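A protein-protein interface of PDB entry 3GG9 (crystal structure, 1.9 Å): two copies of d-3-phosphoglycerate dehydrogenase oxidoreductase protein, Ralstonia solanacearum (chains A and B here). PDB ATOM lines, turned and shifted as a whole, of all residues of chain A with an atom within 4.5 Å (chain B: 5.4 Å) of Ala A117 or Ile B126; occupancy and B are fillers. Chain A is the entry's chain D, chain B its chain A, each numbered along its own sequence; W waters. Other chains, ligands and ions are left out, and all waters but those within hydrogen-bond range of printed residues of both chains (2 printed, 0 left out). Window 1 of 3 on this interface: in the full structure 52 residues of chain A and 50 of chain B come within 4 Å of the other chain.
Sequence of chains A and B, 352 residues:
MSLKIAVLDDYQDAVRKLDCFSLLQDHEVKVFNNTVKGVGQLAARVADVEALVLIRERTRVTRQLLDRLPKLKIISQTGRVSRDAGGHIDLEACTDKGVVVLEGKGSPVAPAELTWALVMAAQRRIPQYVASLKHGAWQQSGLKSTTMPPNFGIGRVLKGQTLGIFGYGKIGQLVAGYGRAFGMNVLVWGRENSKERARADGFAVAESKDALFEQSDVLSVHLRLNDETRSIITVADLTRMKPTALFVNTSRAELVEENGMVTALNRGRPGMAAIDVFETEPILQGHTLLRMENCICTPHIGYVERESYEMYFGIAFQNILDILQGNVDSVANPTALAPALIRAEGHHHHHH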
ATOM      1  N   GLU A 113       9.599   4.154  -3.366  1.00  0.00           N
ATOM      2  CA  GLU A 113      10.122   4.242  -2.015  1.00  0.00           C
ATOM      3  C   GLU A 113      11.434   5.037  -2.014  1.00  0.00           C
ATOM      4  O   GLU A 113      11.654   5.841  -1.116  1.00  0.00           O
ATOM      5  CB  GLU A 113      10.312   2.872  -1.402  1.00  0.00           C
ATOM      6  CG  GLU A 113       8.966   2.148  -1.118  1.00  0.00           C
ATOM      7  CD  GLU A 113       9.128   0.888  -0.303  1.00  0.00           C
ATOM      8  OE1 GLU A 113      10.267   0.542   0.088  1.00  0.00           O
ATOM      9  OE2 GLU A 113       8.107   0.230  -0.027  1.00  0.00           O
ATOM     10  N   LEU A 114      12.260   4.851  -3.040  1.00  0.00           N
ATOM     11  CA  LEU A 114      13.509   5.630  -3.173  1.00  0.00           C
ATOM     12  C   LEU A 114      13.187   7.120  -3.335  1.00  0.00           C
ATOM     13  O   LEU A 114      13.886   7.996  -2.808  1.00  0.00           O
ATOM     14  CB  LEU A 114      14.322   5.161  -4.381  1.00  0.00           C
ATOM     15  CG  LEU A 114      15.793   5.631  -4.511  1.00  0.00           C
ATOM     16  CD1 LEU A 114      15.929   6.915  -5.342  1.00  0.00           C
ATOM     17  CD2 LEU A 114      16.510   5.797  -3.152  1.00  0.00           C
ATOM     18  N   THR A 115      12.149   7.425  -4.103  1.00  0.00           N
ATOM     19  CA  THR A 115      11.736   8.825  -4.225  1.00  0.00           C
ATOM     20  C   THR A 115      11.433   9.385  -2.847  1.00  0.00           C
ATOM     21  O   THR A 115      11.900  10.489  -2.507  1.00  0.00           O
ATOM     22  CB  THR A 115      10.448   8.969  -5.107  1.00  0.00           C
ATOM     23  OG1 THR A 115      10.672   8.387  -6.390  1.00  0.00           O
ATOM     24  CG2 THR A 115      10.072  10.424  -5.280  1.00  0.00           C
ATOM     25  N   TRP A 116      10.630   8.663  -2.051  1.00  0.00           N
ATOM     26  CA  TRP A 116      10.309   9.168  -0.726  1.00  0.00           C
ATOM     27  C   TRP A 116      11.518   9.254   0.200  1.00  0.00           C
ATOM     28  O   TRP A 116      11.665  10.196   0.959  1.00  0.00           O
ATOM     29  CB  TRP A 116       9.181   8.370  -0.056  1.00  0.00           C
ATOM     30  CG  TRP A 116       8.438   9.236   0.909  1.00  0.00           C
ATOM     31  CD1 TRP A 116       8.446   9.158   2.276  1.00  0.00           C
ATOM     32  CD2 TRP A 116       7.588  10.346   0.568  1.00  0.00           C
ATOM     33  NE1 TRP A 116       7.636  10.148   2.808  1.00  0.00           N
ATOM     34  CE2 TRP A 116       7.115  10.900   1.783  1.00  0.00           C
ATOM     35  CE3 TRP A 116       7.203  10.934  -0.646  1.00  0.00           C
ATOM     36  CZ2 TRP A 116       6.242  12.004   1.817  1.00  0.00           C
ATOM     37  CZ3 TRP A 116       6.361  12.053  -0.619  1.00  0.00           C
ATOM     38  CH2 TRP A 116       5.876  12.562   0.604  1.00  0.00           C
ATOM     39  N   ALA A 117      12.389   8.270   0.110  1.00  0.00           N
ATOM     40  CA  ALA A 117      13.644   8.300   0.853  1.00  0.00           C
ATOM     41  C   ALA A 117      14.458   9.590   0.551  1.00  0.00           C
ATOM     42  O   ALA A 117      14.991  10.197   1.476  1.00  0.00           O
ATOM     43  CB  ALA A 117      14.461   7.050   0.538  1.00  0.00           C
ATOM     44  N   LEU A 118      14.544  10.005  -0.722  1.00  0.00           N
ATOM     45  CA  LEU A 118      15.189  11.279  -1.073  1.00  0.00           C
ATOM     46  C   LEU A 118      14.420  12.509  -0.577  1.00  0.00           C
ATOM     47  O   LEU A 118      15.022  13.479  -0.111  1.00  0.00           O
ATOM     48  CB  LEU A 118      15.452  11.406  -2.591  1.00  0.00           C
ATOM     49  CG  LEU A 118      16.482  10.480  -3.238  1.00  0.00           C
ATOM     50  CD1 LEU A 118      16.534  10.626  -4.747  1.00  0.00           C
ATOM     51  CD2 LEU A 118      17.873  10.774  -2.647  1.00  0.00           C
ATOM     52  N   VAL A 119      13.089  12.499  -0.705  1.00  0.00           N
ATOM     53  CA  VAL A 119      12.316  13.612  -0.181  1.00  0.00           C
ATOM     54  C   VAL A 119      12.641  13.807   1.290  1.00  0.00           C
ATOM     55  O   VAL A 119      12.953  14.913   1.699  1.00  0.00           O
ATOM     56  CB  VAL A 119      10.794  13.349  -0.337  1.00  0.00           C
ATOM     57  CG1 VAL A 119       9.982  14.333   0.519  1.00  0.00           C
ATOM     58  CG2 VAL A 119      10.446  13.443  -1.777  1.00  0.00           C
ATOM     59  N   MET A 120      12.651  12.713   2.054  1.00  0.00           N
ATOM     60  CA  MET A 120      12.892  12.796   3.503  1.00  0.00           C
ATOM     61  C   MET A 120      14.346  13.129   3.839  1.00  0.00           C
ATOM     62  O   MET A 120      14.588  13.988   4.705  1.00  0.00           O
ATOM     63  CB  MET A 120      12.412  11.539   4.218  1.00  0.00           C
ATOM     64  CG  MET A 120      10.891  11.371   4.119  1.00  0.00           C
ATOM     65  SD  MET A 120      10.170  10.309   5.370  1.00  0.00           S
ATOM     66  CE  MET A 120      10.058  11.503   6.683  1.00  0.00           C
ATOM     67  N   ALA A 121      15.279  12.504   3.123  1.00  0.00           N
ATOM     68  CA  ALA A 121      16.716  12.772   3.286  1.00  0.00           C
ATOM     69  C   ALA A 121      17.040  14.236   2.997  1.00  0.00           C
ATOM     70  O   ALA A 121      17.808  14.866   3.719  1.00  0.00           O
ATOM     71  CB  ALA A 121      17.556  11.850   2.369  1.00  0.00           C
ATOM     72  N   THR A 298      22.112  10.817  -5.814  1.00  0.00           N
ATOM     73  CA  THR A 298      22.268   9.368  -5.674  1.00  0.00           C
ATOM     74  C   THR A 298      22.525   8.775  -7.052  1.00  0.00           C
ATOM     75  O   THR A 298      22.022   9.297  -8.047  1.00  0.00           O
ATOM     76  CB  THR A 298      21.025   8.705  -5.063  1.00  0.00           C
ATOM     77  OG1 THR A 298      19.865   9.169  -5.765  1.00  0.00           O
ATOM     78  CG2 THR A 298      20.922   9.091  -3.603  1.00  0.00           C
ATOM     79  N   MET B 120      14.169   5.074   6.056  1.00  0.00           N
ATOM     80  CA  MET B 120      14.353   5.122   4.606  1.00  0.00           C
ATOM     81  C   MET B 120      15.821   5.340   4.188  1.00  0.00           C
ATOM     82  O   MET B 120      16.311   4.682   3.268  1.00  0.00           O
ATOM     83  CB  MET B 120      13.406   6.161   4.008  1.00  0.00           C
ATOM     84  CG  MET B 120      11.967   5.789   4.355  1.00  0.00           C
ATOM     85  SD  MET B 120      10.783   6.470   3.207  1.00  0.00           S
ATOM     86  CE  MET B 120      10.826   5.106   2.032  1.00  0.00           C
ATOM     87  N   ALA B 121      16.521   6.221   4.898  1.00  0.00           N
ATOM     88  CA  ALA B 121      17.909   6.528   4.575  1.00  0.00           C
ATOM     89  C   ALA B 121      18.740   5.274   4.772  1.00  0.00           C
ATOM     90  O   ALA B 121      19.490   4.899   3.888  1.00  0.00           O
ATOM     91  CB  ALA B 121      18.426   7.681   5.431  1.00  0.00           C
ATOM     92  N   ALA B 122      18.543   4.593   5.901  1.00  0.00           N
ATOM     93  CA  ALA B 122      19.278   3.348   6.197  1.00  0.00           C
ATOM     94  C   ALA B 122      18.903   2.198   5.256  1.00  0.00           C
ATOM     95  O   ALA B 122      19.767   1.578   4.634  1.00  0.00           O
ATOM     96  CB  ALA B 122      19.073   2.961   7.670  1.00  0.00           C
ATOM     97  N   ARG B 124      17.840   2.194   2.321  1.00  0.00           N
ATOM     98  CA  ARG B 124      18.270   2.413   0.945  1.00  0.00           C
ATOM     99  C   ARG B 124      19.730   2.798   0.842  1.00  0.00           C
ATOM    100  O   ARG B 124      20.211   3.134  -0.256  1.00  0.00           O
ATOM    101  CB  ARG B 124      17.398   3.433   0.207  1.00  0.00           C
ATOM    102  CG  ARG B 124      15.952   2.915  -0.126  1.00  0.00           C
ATOM    103  CD  ARG B 124      15.944   1.532  -0.842  1.00  0.00           C
ATOM    104  NE  ARG B 124      16.207   1.627  -2.285  1.00  0.00           N
ATOM    105  CZ  ARG B 124      15.272   1.650  -3.233  1.00  0.00           C
ATOM    106  NH1 ARG B 124      13.979   1.604  -2.912  1.00  0.00           N
ATOM    107  NH2 ARG B 124      15.646   1.739  -4.506  1.00  0.00           N
ATOM    108  N   ARG B 125      20.404   2.769   1.983  1.00  0.00           N
ATOM    109  CA  ARG B 125      21.864   3.060   2.089  1.00  0.00           C
ATOM    110  C   ARG B 125      22.241   4.412   1.509  1.00  0.00           C
ATOM    111  O   ARG B 125      23.308   4.594   0.925  1.00  0.00           O
ATOM    112  CB  ARG B 125      22.703   1.913   1.508  1.00  0.00           C
ATOM    113  CG  ARG B 125      22.591   0.605   2.299  1.00  0.00           C
ATOM    114  CD  ARG B 125      21.402  -0.269   1.865  1.00  0.00           C
ATOM    115  NE  ARG B 125      21.462  -1.623   2.417  1.00  0.00           N
ATOM    116  CZ  ARG B 125      20.919  -2.017   3.571  1.00  0.00           C
ATOM    117  NH1 ARG B 125      21.029  -3.279   3.935  1.00  0.00           N
ATOM    118  NH2 ARG B 125      20.246  -1.181   4.354  1.00  0.00           N
ATOM    119  N   ILE B 126      21.338   5.373   1.682  1.00  0.00           N
ATOM    120  CA  ILE B 126      21.523   6.689   1.118  1.00  0.00           C
ATOM    121  C   ILE B 126      22.825   7.426   1.531  1.00  0.00           C
ATOM    122  O   ILE B 126      23.531   7.848   0.636  1.00  0.00           O
ATOM    123  CB  ILE B 126      20.271   7.547   1.261  1.00  0.00           C
ATOM    124  CG1 ILE B 126      19.150   6.865   0.482  1.00  0.00           C
ATOM    125  CG2 ILE B 126      20.543   8.986   0.809  1.00  0.00           C
ATOM    126  CD1 ILE B 126      17.887   7.659   0.453  1.00  0.00           C
ATOM    127  N   PRO B 127      23.143   7.552   2.850  1.00  0.00           N
ATOM    128  CA  PRO B 127      24.404   8.224   3.189  1.00  0.00           C
ATOM    129  C   PRO B 127      25.625   7.559   2.536  1.00  0.00           C
ATOM    130  O   PRO B 127      26.487   8.259   1.988  1.00  0.00           O
ATOM    131  CB  PRO B 127      24.471   8.090   4.718  1.00  0.00           C
ATOM    132  CG  PRO B 127      23.062   7.989   5.134  1.00  0.00           C
ATOM    133  CD  PRO B 127      22.420   7.144   4.078  1.00  0.00           C
ATOM    134  N   GLN B 128      25.667   6.228   2.568  1.00  0.00           N
ATOM    135  CA  GLN B 128      26.769   5.459   1.980  1.00  0.00           C
ATOM    136  C   GLN B 128      26.918   5.646   0.459  1.00  0.00           C
ATOM    137  O   GLN B 128      28.016   5.858  -0.034  1.00  0.00           O
ATOM    138  CB  GLN B 128      26.651   3.970   2.324  1.00  0.00           C
ATOM    139  CG  GLN B 128      26.650   3.648   3.829  1.00  0.00           C
ATOM    140  CD  GLN B 128      25.249   3.562   4.431  1.00  0.00           C
ATOM    141  OE1 GLN B 128      24.293   4.186   3.941  1.00  0.00           O
ATOM    142  NE2 GLN B 128      25.118   2.771   5.489  1.00  0.00           N
ATOM    143  N   TYR B 129      25.815   5.574  -0.272  1.00  0.00           N
ATOM    144  CA  TYR B 129      25.863   5.744  -1.711  1.00  0.00           C
ATOM    145  C   TYR B 129      26.219   7.183  -2.082  1.00  0.00           C
ATOM    146  O   TYR B 129      26.962   7.406  -3.038  1.00  0.00           O
ATOM    147  CB  TYR B 129      24.505   5.418  -2.337  1.00  0.00           C
ATOM    148  CG  TYR B 129      24.236   3.984  -2.744  1.00  0.00           C
ATOM    149  CD1 TYR B 129      24.941   3.373  -3.794  1.00  0.00           C
ATOM    150  CD2 TYR B 129      23.199   3.272  -2.144  1.00  0.00           C
ATOM    151  CE1 TYR B 129      24.644   2.044  -4.196  1.00  0.00           C
ATOM    152  CE2 TYR B 129      22.899   1.969  -2.533  1.00  0.00           C
ATOM    153  CZ  TYR B 129      23.616   1.365  -3.558  1.00  0.00           C
ATOM    154  OH  TYR B 129      23.259   0.076  -3.909  1.00  0.00           O
ATOM    155  N   VAL B 130      25.668   8.153  -1.343  1.00  0.00           N
ATOM    156  CA  VAL B 130      25.891   9.580  -1.623  1.00  0.00           C
ATOM    157  C   VAL B 130      27.378   9.944  -1.427  1.00  0.00           C
ATOM    158  O   VAL B 130      27.980  10.612  -2.280  1.00  0.00           O
ATOM    159  CB  VAL B 130      25.018  10.481  -0.730  1.00  0.00           C
ATOM    160  CG1 VAL B 130      25.538  11.915  -0.707  1.00  0.00           C
ATOM    161  CG2 VAL B 130      23.570  10.449  -1.210  1.00  0.00           C
ATOM    162  N   ALA B 131      27.946   9.486  -0.316  1.00  0.00           N
ATOM    163  CA  ALA B 131      29.340   9.777   0.033  1.00  0.00           C
ATOM    164  C   ALA B 131      30.336   9.133  -0.934  1.00  0.00           C
ATOM    165  O   ALA B 131      31.365   9.733  -1.271  1.00  0.00           O
ATOM    166  CB  ALA B 131      29.628   9.311   1.445  1.00  0.00           C
HETATM  167  O   HOH W   1      15.999   9.474   4.105  1.00  0.00           O
HETATM  168  O   HOH W   2      12.845   0.943  -0.219  1.00  0.00           O
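Of the 11 printed residues of chain B, 4 touch a printed residue of chain A.
Printed residues of chain B that touch a printed residue of chain A: Met B120, Arg B124, Ile B126 and Val B130.
Hydrophobic or aromatic side chains of chain B within 4 Å of the printed part of chain A: Met B120, Ile B126 and Val B130.
Along chain B the printed residues that touch a printed residue of chain A span positions 120 to 130.
Among the printed residues, no Asp or Glu carboxylate lies within 4 Å of a Lys or Arg side-chain nitrogen of the other chain.
The side-chain sulfur (SD) of Met A120 sits at hydrogen-bond distance from the indole nitrogen (NE1) of Trp A116 (3.6 Å).
N of Ile B126 is in hydrogen-bond range of O of Ala B121 (2.9 Å).
2 positions are printed for both chains.
Of the 6 pairs that touch across the chains among the printed residues, none has its exchanged pair printed and touching as well.
Thr A115 touches none of the printed residues of chain B.
Of chain B, only Met B120 (3.7 Å) and Ile B126 (3.5 Å) come within 4 Å of Ala A117.
Of the printed residues of chain A, Met B120 touches Glu A113 (3.3 Å), Trp A116 (3.7 Å) and Ala A117 (3.7 Å).
Printed residues of chain A within 4 Å of Arg B124: Leu A114 (3.7 Å).
Of the printed residues of chain A, Ile B126 touches Ala A117 (3.5 Å).
Printed residues of chain A within 4 Å of Val B130: Thr A298.
The nearest residue of chain B that does not touch Ala A117 is Arg B124 (4.4 Å).
Water W2 bridges OE1 of Glu A113 (2.6 Å) and NH1 of Arg B124 (3.0 Å).
Water W1 lies within hydrogen-bond range of the backbone carbonyl oxygen (O) of Ala A117 (2.9 Å), the backbone NH (N) of Ala A121 (3.3 Å) and the backbone NH (N) of Ala B121 (3.4 Å).
Among the printed residues, merely in contact across the chains: Glu A113 with Met B120 (3.3 Å), Leu A114 with Arg B124 (3.7 Å), Trp A116 with Met B120 (3.7 Å), Ala A117 with Met B120 (3.7 Å), Ala A117 with Ile B126 (3.5 Å) and Thr A298 with Val B130 (3.8 Å).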
